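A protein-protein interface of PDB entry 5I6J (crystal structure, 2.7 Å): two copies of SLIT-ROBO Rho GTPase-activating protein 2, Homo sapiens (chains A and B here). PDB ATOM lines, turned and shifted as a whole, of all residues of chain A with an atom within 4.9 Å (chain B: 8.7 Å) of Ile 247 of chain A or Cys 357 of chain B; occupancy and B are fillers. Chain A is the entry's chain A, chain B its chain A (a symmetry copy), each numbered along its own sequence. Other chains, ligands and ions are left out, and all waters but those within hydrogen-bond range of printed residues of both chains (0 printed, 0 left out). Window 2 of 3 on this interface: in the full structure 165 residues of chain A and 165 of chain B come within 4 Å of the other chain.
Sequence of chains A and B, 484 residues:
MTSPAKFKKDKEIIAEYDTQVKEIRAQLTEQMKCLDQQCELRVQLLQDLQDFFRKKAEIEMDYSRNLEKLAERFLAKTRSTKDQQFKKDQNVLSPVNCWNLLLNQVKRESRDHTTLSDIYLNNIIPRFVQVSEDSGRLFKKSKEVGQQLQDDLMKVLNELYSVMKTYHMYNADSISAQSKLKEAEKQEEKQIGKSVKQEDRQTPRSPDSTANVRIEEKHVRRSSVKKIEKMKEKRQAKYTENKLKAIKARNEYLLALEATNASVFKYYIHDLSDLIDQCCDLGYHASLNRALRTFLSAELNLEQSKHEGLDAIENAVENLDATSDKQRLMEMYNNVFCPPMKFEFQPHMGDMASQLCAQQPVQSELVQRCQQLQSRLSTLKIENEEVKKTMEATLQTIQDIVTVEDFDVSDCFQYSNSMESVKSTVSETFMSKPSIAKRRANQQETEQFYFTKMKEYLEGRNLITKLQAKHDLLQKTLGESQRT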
ATOM      1  N   LYS A 243      21.643 -22.701  23.690  1.00  0.00           N
ATOM      2  CA  LYS A 243      21.744 -21.362  24.291  1.00  0.00           C
ATOM      3  C   LYS A 243      22.625 -20.429  23.455  1.00  0.00           C
ATOM      4  O   LYS A 243      22.415 -19.218  23.458  1.00  0.00           O
ATOM      5  CB  LYS A 243      22.226 -21.413  25.746  1.00  0.00           C
ATOM      6  CG  LYS A 243      21.552 -20.391  26.665  1.00  0.00           C
ATOM      7  CD  LYS A 243      22.296 -19.055  26.739  1.00  0.00           C
ATOM      8  CE  LYS A 243      21.360 -17.856  26.567  1.00  0.00           C
ATOM      9  NZ  LYS A 243      20.592 -17.455  27.779  1.00  0.00           N
ATOM     10  N   LEU A 244      23.607 -20.998  22.755  1.00  0.00           N
ATOM     11  CA  LEU A 244      24.377 -20.265  21.751  1.00  0.00           C
ATOM     12  C   LEU A 244      23.496 -19.850  20.556  1.00  0.00           C
ATOM     13  O   LEU A 244      23.569 -18.703  20.101  1.00  0.00           O
ATOM     14  CB  LEU A 244      25.565 -21.106  21.277  1.00  0.00           C
ATOM     15  CG  LEU A 244      26.637 -20.455  20.398  1.00  0.00           C
ATOM     16  CD1 LEU A 244      27.678 -19.787  21.291  1.00  0.00           C
ATOM     17  CD2 LEU A 244      27.276 -21.477  19.460  1.00  0.00           C
ATOM     18  N   LYS A 245      22.682 -20.793  20.059  1.00  0.00           N
ATOM     19  CA  LYS A 245      21.721 -20.563  18.965  1.00  0.00           C
ATOM     20  C   LYS A 245      20.763 -19.426  19.281  1.00  0.00           C
ATOM     21  O   LYS A 245      20.499 -18.602  18.412  1.00  0.00           O
ATOM     22  CB  LYS A 245      20.911 -21.829  18.622  1.00  0.00           C
ATOM     23  CG  LYS A 245      21.618 -22.845  17.723  1.00  0.00           C
ATOM     24  CD  LYS A 245      20.698 -23.456  16.656  1.00  0.00           C
ATOM     25  CE  LYS A 245      19.641 -24.416  17.203  1.00  0.00           C
ATOM     26  NZ  LYS A 245      20.150 -25.787  17.446  1.00  0.00           N
ATOM     27  N   ALA A 246      20.262 -19.387  20.519  1.00  0.00           N
ATOM     28  CA  ALA A 246      19.394 -18.298  20.996  1.00  0.00           C
ATOM     29  C   ALA A 246      20.095 -16.942  20.945  1.00  0.00           C
ATOM     30  O   ALA A 246      19.522 -15.971  20.447  1.00  0.00           O
ATOM     31  CB  ALA A 246      18.867 -18.568  22.408  1.00  0.00           C
ATOM     32  N   ILE A 247      21.326 -16.889  21.453  1.00  0.00           N
ATOM     33  CA  ILE A 247      22.133 -15.671  21.470  1.00  0.00           C
ATOM     34  C   ILE A 247      22.341 -15.190  20.034  1.00  0.00           C
ATOM     35  O   ILE A 247      22.113 -14.011  19.737  1.00  0.00           O
ATOM     36  CB  ILE A 247      23.480 -15.866  22.257  1.00  0.00           C
ATOM     37  CG1 ILE A 247      23.250 -15.683  23.773  1.00  0.00           C
ATOM     38  CG2 ILE A 247      24.592 -14.922  21.775  1.00  0.00           C
ATOM     39  CD1 ILE A 247      24.471 -15.872  24.657  1.00  0.00           C
ATOM     40  N   LYS A 248      22.744 -16.103  19.147  1.00  0.00           N
ATOM     41  CA  LYS A 248      23.036 -15.735  17.770  1.00  0.00           C
ATOM     42  C   LYS A 248      21.790 -15.221  17.041  1.00  0.00           C
ATOM     43  O   LYS A 248      21.882 -14.260  16.273  1.00  0.00           O
ATOM     44  CB  LYS A 248      23.729 -16.866  17.018  1.00  0.00           C
ATOM     45  CG  LYS A 248      25.242 -16.867  17.221  1.00  0.00           C
ATOM     46  CD  LYS A 248      25.971 -17.830  16.286  1.00  0.00           C
ATOM     47  CE  LYS A 248      25.843 -19.273  16.761  1.00  0.00           C
ATOM     48  NZ  LYS A 248      26.805 -20.191  16.098  1.00  0.00           N
ATOM     49  N   ALA A 249      20.635 -15.828  17.317  1.00  0.00           N
ATOM     50  CA  ALA A 249      19.367 -15.334  16.783  1.00  0.00           C
ATOM     51  C   ALA A 249      18.879 -14.020  17.419  1.00  0.00           C
ATOM     52  O   ALA A 249      18.312 -13.181  16.716  1.00  0.00           O
ATOM     53  CB  ALA A 249      18.282 -16.397  16.844  1.00  0.00           C
ATOM     54  N   ARG A 250      19.073 -13.839  18.725  1.00  0.00           N
ATOM     55  CA  ARG A 250      18.662 -12.598  19.392  1.00  0.00           C
ATOM     56  C   ARG A 250      19.494 -11.382  18.897  1.00  0.00           C
ATOM     57  O   ARG A 250      18.985 -10.255  18.745  1.00  0.00           O
ATOM     58  CB  ARG A 250      18.743 -12.742  20.908  1.00  0.00           C
ATOM     59  CG  ARG A 250      18.106 -11.588  21.674  1.00  0.00           C
ATOM     60  CD  ARG A 250      18.745 -11.350  23.047  1.00  0.00           C
ATOM     61  NE  ARG A 250      18.302 -12.333  24.040  1.00  0.00           N
ATOM     62  CZ  ARG A 250      19.056 -13.308  24.527  1.00  0.00           C
ATOM     63  NH1 ARG A 250      20.321 -13.440  24.146  1.00  0.00           N
ATOM     64  NH2 ARG A 250      18.541 -14.152  25.401  1.00  0.00           N
ATOM     65  N   ASN A 251      20.768 -11.629  18.625  1.00  0.00           N
ATOM     66  CA  ASN A 251      21.647 -10.593  18.144  1.00  0.00           C
ATOM     67  C   ASN A 251      21.227 -10.163  16.726  1.00  0.00           C
ATOM     68  O   ASN A 251      21.298  -8.985  16.386  1.00  0.00           O
ATOM     69  CB  ASN A 251      23.100 -11.081  18.197  1.00  0.00           C
ATOM     70  CG  ASN A 251      23.775 -10.879  19.574  1.00  0.00           C
ATOM     71  OD1 ASN A 251      23.171 -10.463  20.587  1.00  0.00           O
ATOM     72  ND2 ASN A 251      25.066 -11.179  19.599  1.00  0.00           N
ATOM     73  N   ASP B 351      12.489 -12.837  28.663  1.00  0.00           N
ATOM     74  CA  ASP B 351      13.945 -12.754  28.528  1.00  0.00           C
ATOM     75  C   ASP B 351      14.582 -11.689  29.432  1.00  0.00           C
ATOM     76  O   ASP B 351      14.046 -10.591  29.586  1.00  0.00           O
ATOM     77  CB  ASP B 351      14.289 -12.456  27.064  1.00  0.00           C
ATOM     78  CG  ASP B 351      15.709 -12.878  26.678  1.00  0.00           C
ATOM     79  OD1 ASP B 351      16.690 -12.545  27.400  1.00  0.00           O
ATOM     80  OD2 ASP B 351      15.835 -13.519  25.612  1.00  0.00           O
ATOM     81  N   ALA B 353      18.145 -10.470  29.538  1.00  0.00           N
ATOM     82  CA  ALA B 353      19.005  -9.515  28.811  1.00  0.00           C
ATOM     83  C   ALA B 353      18.319  -9.075  27.512  1.00  0.00           C
ATOM     84  O   ALA B 353      17.407  -9.749  27.034  1.00  0.00           O
ATOM     85  CB  ALA B 353      20.376 -10.120  28.526  1.00  0.00           C
ATOM     86  N   SER B 354      18.745  -7.939  26.957  1.00  0.00           N
ATOM     87  CA  SER B 354      18.051  -7.335  25.816  1.00  0.00           C
ATOM     88  C   SER B 354      18.947  -6.354  25.064  1.00  0.00           C
ATOM     89  O   SER B 354      18.483  -5.352  24.513  1.00  0.00           O
ATOM     90  CB  SER B 354      16.799  -6.616  26.303  1.00  0.00           C
ATOM     91  OG  SER B 354      17.173  -5.479  27.044  1.00  0.00           O
ATOM     92  N   GLN B 355      20.238  -6.655  25.064  1.00  0.00           N
ATOM     93  CA  GLN B 355      21.258  -5.881  24.359  1.00  0.00           C
ATOM     94  C   GLN B 355      22.060  -6.887  23.517  1.00  0.00           C
ATOM     95  O   GLN B 355      21.812  -8.096  23.585  1.00  0.00           O
ATOM     96  CB  GLN B 355      22.177  -5.149  25.367  1.00  0.00           C
ATOM     97  CG  GLN B 355      21.486  -4.463  26.552  1.00  0.00           C
ATOM     98  CD  GLN B 355      22.189  -4.720  27.890  1.00  0.00           C
ATOM     99  OE1 GLN B 355      22.764  -3.803  28.487  1.00  0.00           O
ATOM    100  NE2 GLN B 355      22.143  -5.976  28.366  1.00  0.00           N
ATOM    101  N   LEU B 356      23.003  -6.403  22.714  1.00  0.00           N
ATOM    102  CA  LEU B 356      23.937  -7.293  22.048  1.00  0.00           C
ATOM    103  C   LEU B 356      24.735  -8.050  23.093  1.00  0.00           C
ATOM    104  O   LEU B 356      25.277  -7.434  24.014  1.00  0.00           O
ATOM    105  CB  LEU B 356      24.905  -6.520  21.157  1.00  0.00           C
ATOM    106  CG  LEU B 356      24.442  -6.047  19.779  1.00  0.00           C
ATOM    107  CD1 LEU B 356      25.622  -5.448  19.031  1.00  0.00           C
ATOM    108  CD2 LEU B 356      23.807  -7.152  18.947  1.00  0.00           C
ATOM    109  N   CYS B 357      24.761  -9.380  22.962  1.00  0.00           N
ATOM    110  CA  CYS B 357      25.632 -10.229  23.760  1.00  0.00           C
ATOM    111  C   CYS B 357      26.917 -10.535  22.971  1.00  0.00           C
ATOM    112  O   CYS B 357      26.882 -11.291  21.999  1.00  0.00           O
ATOM    113  CB  CYS B 357      24.900 -11.512  24.171  1.00  0.00           C
ATOM    114  SG  CYS B 357      25.691 -12.403  25.534  1.00  0.00           S
ATOM    115  N   ALA B 358      28.038  -9.924  23.380  1.00  0.00           N
ATOM    116  CA  ALA B 358      29.358 -10.137  22.735  1.00  0.00           C
ATOM    117  C   ALA B 358      30.299 -11.052  23.542  1.00  0.00           C
ATOM    118  O   ALA B 358      31.508 -10.807  23.637  1.00  0.00           O
ATOM    119  CB  ALA B 358      30.030  -8.812  22.392  1.00  0.00           C
ATOM    120  N   GLN B 359      29.713 -12.122  24.088  1.00  0.00           N
ATOM    121  CA  GLN B 359      30.402 -13.182  24.836  1.00  0.00           C
ATOM    122  C   GLN B 359      31.346 -14.011  23.941  1.00  0.00           C
ATOM    123  O   GLN B 359      31.634 -13.628  22.805  1.00  0.00           O
ATOM    124  CB  GLN B 359      29.343 -14.077  25.488  1.00  0.00           C
ATOM    125  CG  GLN B 359      29.638 -14.439  26.936  1.00  0.00           C
ATOM    126  CD  GLN B 359      28.420 -14.966  27.676  1.00  0.00           C
ATOM    127  OE1 GLN B 359      27.940 -16.070  27.410  1.00  0.00           O
ATOM    128  NE2 GLN B 359      27.919 -14.177  28.621  1.00  0.00           N
ATOM    129  N   GLN B 360      31.834 -15.134  24.460  1.00  0.00           N
ATOM    130  CA  GLN B 360      32.685 -16.068  23.716  1.00  0.00           C
ATOM    131  C   GLN B 360      31.805 -17.179  23.125  1.00  0.00           C
ATOM    132  O   GLN B 360      30.844 -17.575  23.784  1.00  0.00           O
ATOM    133  CB  GLN B 360      33.728 -16.666  24.673  1.00  0.00           C
ATOM    134  CG  GLN B 360      35.144 -16.745  24.119  1.00  0.00           C
ATOM    135  CD  GLN B 360      35.636 -15.412  23.574  1.00  0.00           C
ATOM    136  OE1 GLN B 360      35.776 -15.249  22.362  1.00  0.00           O
ATOM    137  NE2 GLN B 360      35.875 -14.446  24.464  1.00  0.00           N
ATOM    138  N   PRO B 361      32.082 -17.689  21.915  1.00  0.00           N
ATOM    139  CA  PRO B 361      33.195 -17.275  21.044  1.00  0.00           C
ATOM    140  C   PRO B 361      32.794 -16.191  20.037  1.00  0.00           C
ATOM    141  O   PRO B 361      33.588 -15.841  19.145  1.00  0.00           O
ATOM    142  CB  PRO B 361      33.524 -18.572  20.291  1.00  0.00           C
ATOM    143  CG  PRO B 361      32.200 -19.275  20.168  1.00  0.00           C
ATOM    144  CD  PRO B 361      31.359 -18.852  21.351  1.00  0.00           C
ATOM    145  N   VAL B 362      31.577 -15.669  20.210  1.00  0.00           N
ATOM    146  CA  VAL B 362      30.902 -14.839  19.216  1.00  0.00           C
ATOM    147  C   VAL B 362      31.576 -13.479  18.996  1.00  0.00           C
ATOM    148  O   VAL B 362      31.482 -12.897  17.910  1.00  0.00           O
ATOM    149  CB  VAL B 362      29.379 -14.766  19.492  1.00  0.00           C
ATOM    150  CG1 VAL B 362      29.065 -13.959  20.736  1.00  0.00           C
ATOM    151  CG2 VAL B 362      28.622 -14.229  18.284  1.00  0.00           C
ATOM    152  N   GLN B 363      32.296 -13.012  20.012  1.00  0.00           N
ATOM    153  CA  GLN B 363      33.052 -11.772  19.921  1.00  0.00           C
ATOM    154  C   GLN B 363      33.931 -11.721  18.658  1.00  0.00           C
ATOM    155  O   GLN B 363      33.981 -10.693  17.985  1.00  0.00           O
ATOM    156  CB  GLN B 363      33.874 -11.539  21.194  1.00  0.00           C
ATOM    157  CG  GLN B 363      34.284 -10.093  21.421  1.00  0.00           C
ATOM    158  CD  GLN B 363      34.392  -9.723  22.893  1.00  0.00           C
ATOM    159  OE1 GLN B 363      33.686  -8.824  23.375  1.00  0.00           O
ATOM    160  NE2 GLN B 363      35.277 -10.410  23.618  1.00  0.00           N
ATOM    161  N   SER B 364      34.583 -12.828  18.314  1.00  0.00           N
ATOM    162  CA  SER B 364      35.465 -12.857  17.143  1.00  0.00           C
ATOM    163  C   SER B 364      34.712 -12.782  15.815  1.00  0.00           C
ATOM    164  O   SER B 364      35.252 -12.260  14.852  1.00  0.00           O
ATOM    165  CB  SER B 364      36.355 -14.088  17.174  1.00  0.00           C
ATOM    166  OG  SER B 364      35.557 -15.255  17.193  1.00  0.00           O
ATOM    167  N   GLU B 365      33.485 -13.308  15.771  1.00  0.00           N
ATOM    168  CA  GLU B 365      32.601 -13.209  14.589  1.00  0.00           C
ATOM    169  C   GLU B 365      32.033 -11.803  14.443  1.00  0.00           C
ATOM    170  O   GLU B 365      31.999 -11.262  13.344  1.00  0.00           O
ATOM    171  CB  GLU B 365      31.420 -14.172  14.683  1.00  0.00           C
ATOM    172  CG  GLU B 365      31.760 -15.650  14.655  1.00  0.00           C
ATOM    173  CD  GLU B 365      30.987 -16.428  15.713  1.00  0.00           C
ATOM    174  OE1 GLU B 365      31.635 -16.925  16.668  1.00  0.00           O
ATOM    175  OE2 GLU B 365      29.739 -16.528  15.612  1.00  0.00           O
ATOM    176  N   LEU B 366      31.561 -11.239  15.554  1.00  0.00           N
ATOM    177  CA  LEU B 366      31.041  -9.876  15.617  1.00  0.00           C
ATOM    178  C   LEU B 366      32.080  -8.801  15.280  1.00  0.00           C
ATOM    179  O   LEU B 366      31.734  -7.738  14.768  1.00  0.00           O
ATOM    180  CB  LEU B 366      30.448  -9.598  16.992  1.00  0.00           C
ATOM    181  CG  LEU B 366      29.198 -10.350  17.465  1.00  0.00           C
ATOM    182  CD1 LEU B 366      28.886  -9.961  18.909  1.00  0.00           C
ATOM    183  CD2 LEU B 366      27.971 -10.142  16.580  1.00  0.00           C
ATOM    184  N   LEU B 473      25.566  -0.174  16.013  1.00  0.00           N
ATOM    185  CA  LEU B 473      25.188  -0.986  17.183  1.00  0.00           C
ATOM    186  C   LEU B 473      26.334  -1.915  17.587  1.00  0.00           C
ATOM    187  O   LEU B 473      26.554  -2.124  18.790  1.00  0.00           O
ATOM    188  CB  LEU B 473      23.877  -1.781  17.007  1.00  0.00           C
ATOM    189  CG  LEU B 473      23.252  -2.244  18.352  1.00  0.00           C
ATOM    190  CD1 LEU B 473      22.547  -1.113  19.110  1.00  0.00           C
ATOM    191  CD2 LEU B 473      22.288  -3.413  18.209  1.00  0.00           C
ATOM    192  N   LEU B 474      27.054  -2.458  16.597  1.00  0.00           N
ATOM    193  CA  LEU B 474      28.214  -3.305  16.882  1.00  0.00           C
ATOM    194  C   LEU B 474      29.348  -2.487  17.519  1.00  0.00           C
ATOM    195  O   LEU B 474      29.834  -2.843  18.592  1.00  0.00           O
ATOM    196  CB  LEU B 474      28.717  -4.094  15.650  1.00  0.00           C
ATOM    197  CG  LEU B 474      27.871  -5.151  14.904  1.00  0.00           C
ATOM    198  CD1 LEU B 474      28.666  -5.739  13.745  1.00  0.00           C
ATOM    199  CD2 LEU B 474      27.295  -6.276  15.758  1.00  0.00           C
ATOM    200  N   THR B 477      29.048  -1.602  21.203  1.00  0.00           N
ATOM    201  CA  THR B 477      29.211  -2.858  21.963  1.00  0.00           C
ATOM    202  C   THR B 477      30.669  -3.375  22.137  1.00  0.00           C
ATOM    203  O   THR B 477      31.052  -3.754  23.254  1.00  0.00           O
ATOM    204  CB  THR B 477      28.302  -3.965  21.356  1.00  0.00           C
ATOM    205  OG1 THR B 477      27.026  -3.955  22.007  1.00  0.00           O
ATOM    206  CG2 THR B 477      28.912  -5.364  21.483  1.00  0.00           C
ATOM    207  N   LEU B 478      31.443  -3.387  21.045  1.00  0.00           N
ATOM    208  CA  LEU B 478      32.822  -3.911  21.014  1.00  0.00           C
ATOM    209  C   LEU B 478      33.892  -2.856  21.328  1.00  0.00           C
ATOM    210  O   LEU B 478      34.625  -3.015  22.309  1.00  0.00           O
ATOM    211  CB  LEU B 478      33.156  -4.621  19.677  1.00  0.00           C
ATOM    212  CG  LEU B 478      32.187  -5.609  18.982  1.00  0.00           C
ATOM    213  CD1 LEU B 478      32.530  -5.765  17.495  1.00  0.00           C
ATOM    214  CD2 LEU B 478      32.033  -6.962  19.688  1.00  0.00           C
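No position is printed for both chains.
Of the 5 pairs that touch across the chains among the printed residues, none has its exchanged pair printed and touching as well.
The side-chain carboxylate of Asp 351 of chain B sits at hydrogen-bond distance from the backbone NH of Ala 353 of chain B, at 3.3 Å.
OG of Ser 364 of chain B is in hydrogen-bond range of O of Pro 361 of chain B (2.8 Å).
Leu 244 of chain A touches Pro 361 of chain B (CD1 to CD, 3.8 Å).
Cys 357 of chain B touches Ile 247 of chain A.
OD1 of Asn 251 of chain A touches CA of Leu 356 of chain B, at 3.6 Å.
The guanidinium group (NH2) of Arg 250 of chain A lies within salt-bridge range of the side-chain carboxylate (OD2) of Asp 351 of chain B.
The side-chain amide nitrogen (ND2) of Asn 251 of chain A is in hydrogen-bond range of the backbone carbonyl oxygen (O) of Cys 357 of chain B, 3.0 Å away.
Hydrophobic or aromatic side chains of chain A that line the printed part of chain B: Leu 244 and Ile 247.
Of the 19 printed residues of chain B, 4 touch a printed residue of chain A.
Hydrophobic or aromatic side chains of chain B that line the printed part of chain A: Leu 356 and Pro 361.
Ile 247 of chain A touches just one residue of chain B: Cys 357.
Of chain A, only Ile 247 (3.8 Å) and Asn 251 (3.0 Å) come within 4 Å of Cys 357 of chain B.
No residue of chain B comes within 4 Å of Ala 246 of chain A.
Of the printed residues of chain B, Leu 244 of chain A touches Pro 361 (3.8 Å).
Printed residues of chain B within 4 Å of Arg 250 of chain A: Asp 351.
Of the printed residues of chain A, Asp 351 of chain B touches Arg 250 (2.8 Å).
Ala 353 of chain B touches none of the printed residues of chain A.
Leu 478 of chain B touches none of the printed residues of chain A.
The nearest printed residue of chain A that does not touch Cys 357 of chain B is Arg 250 of chain A (5.0 Å).
The nearest printed residue of chain B that does not touch Arg 250 of chain A is Ala 353 of chain B (4.1 Å).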
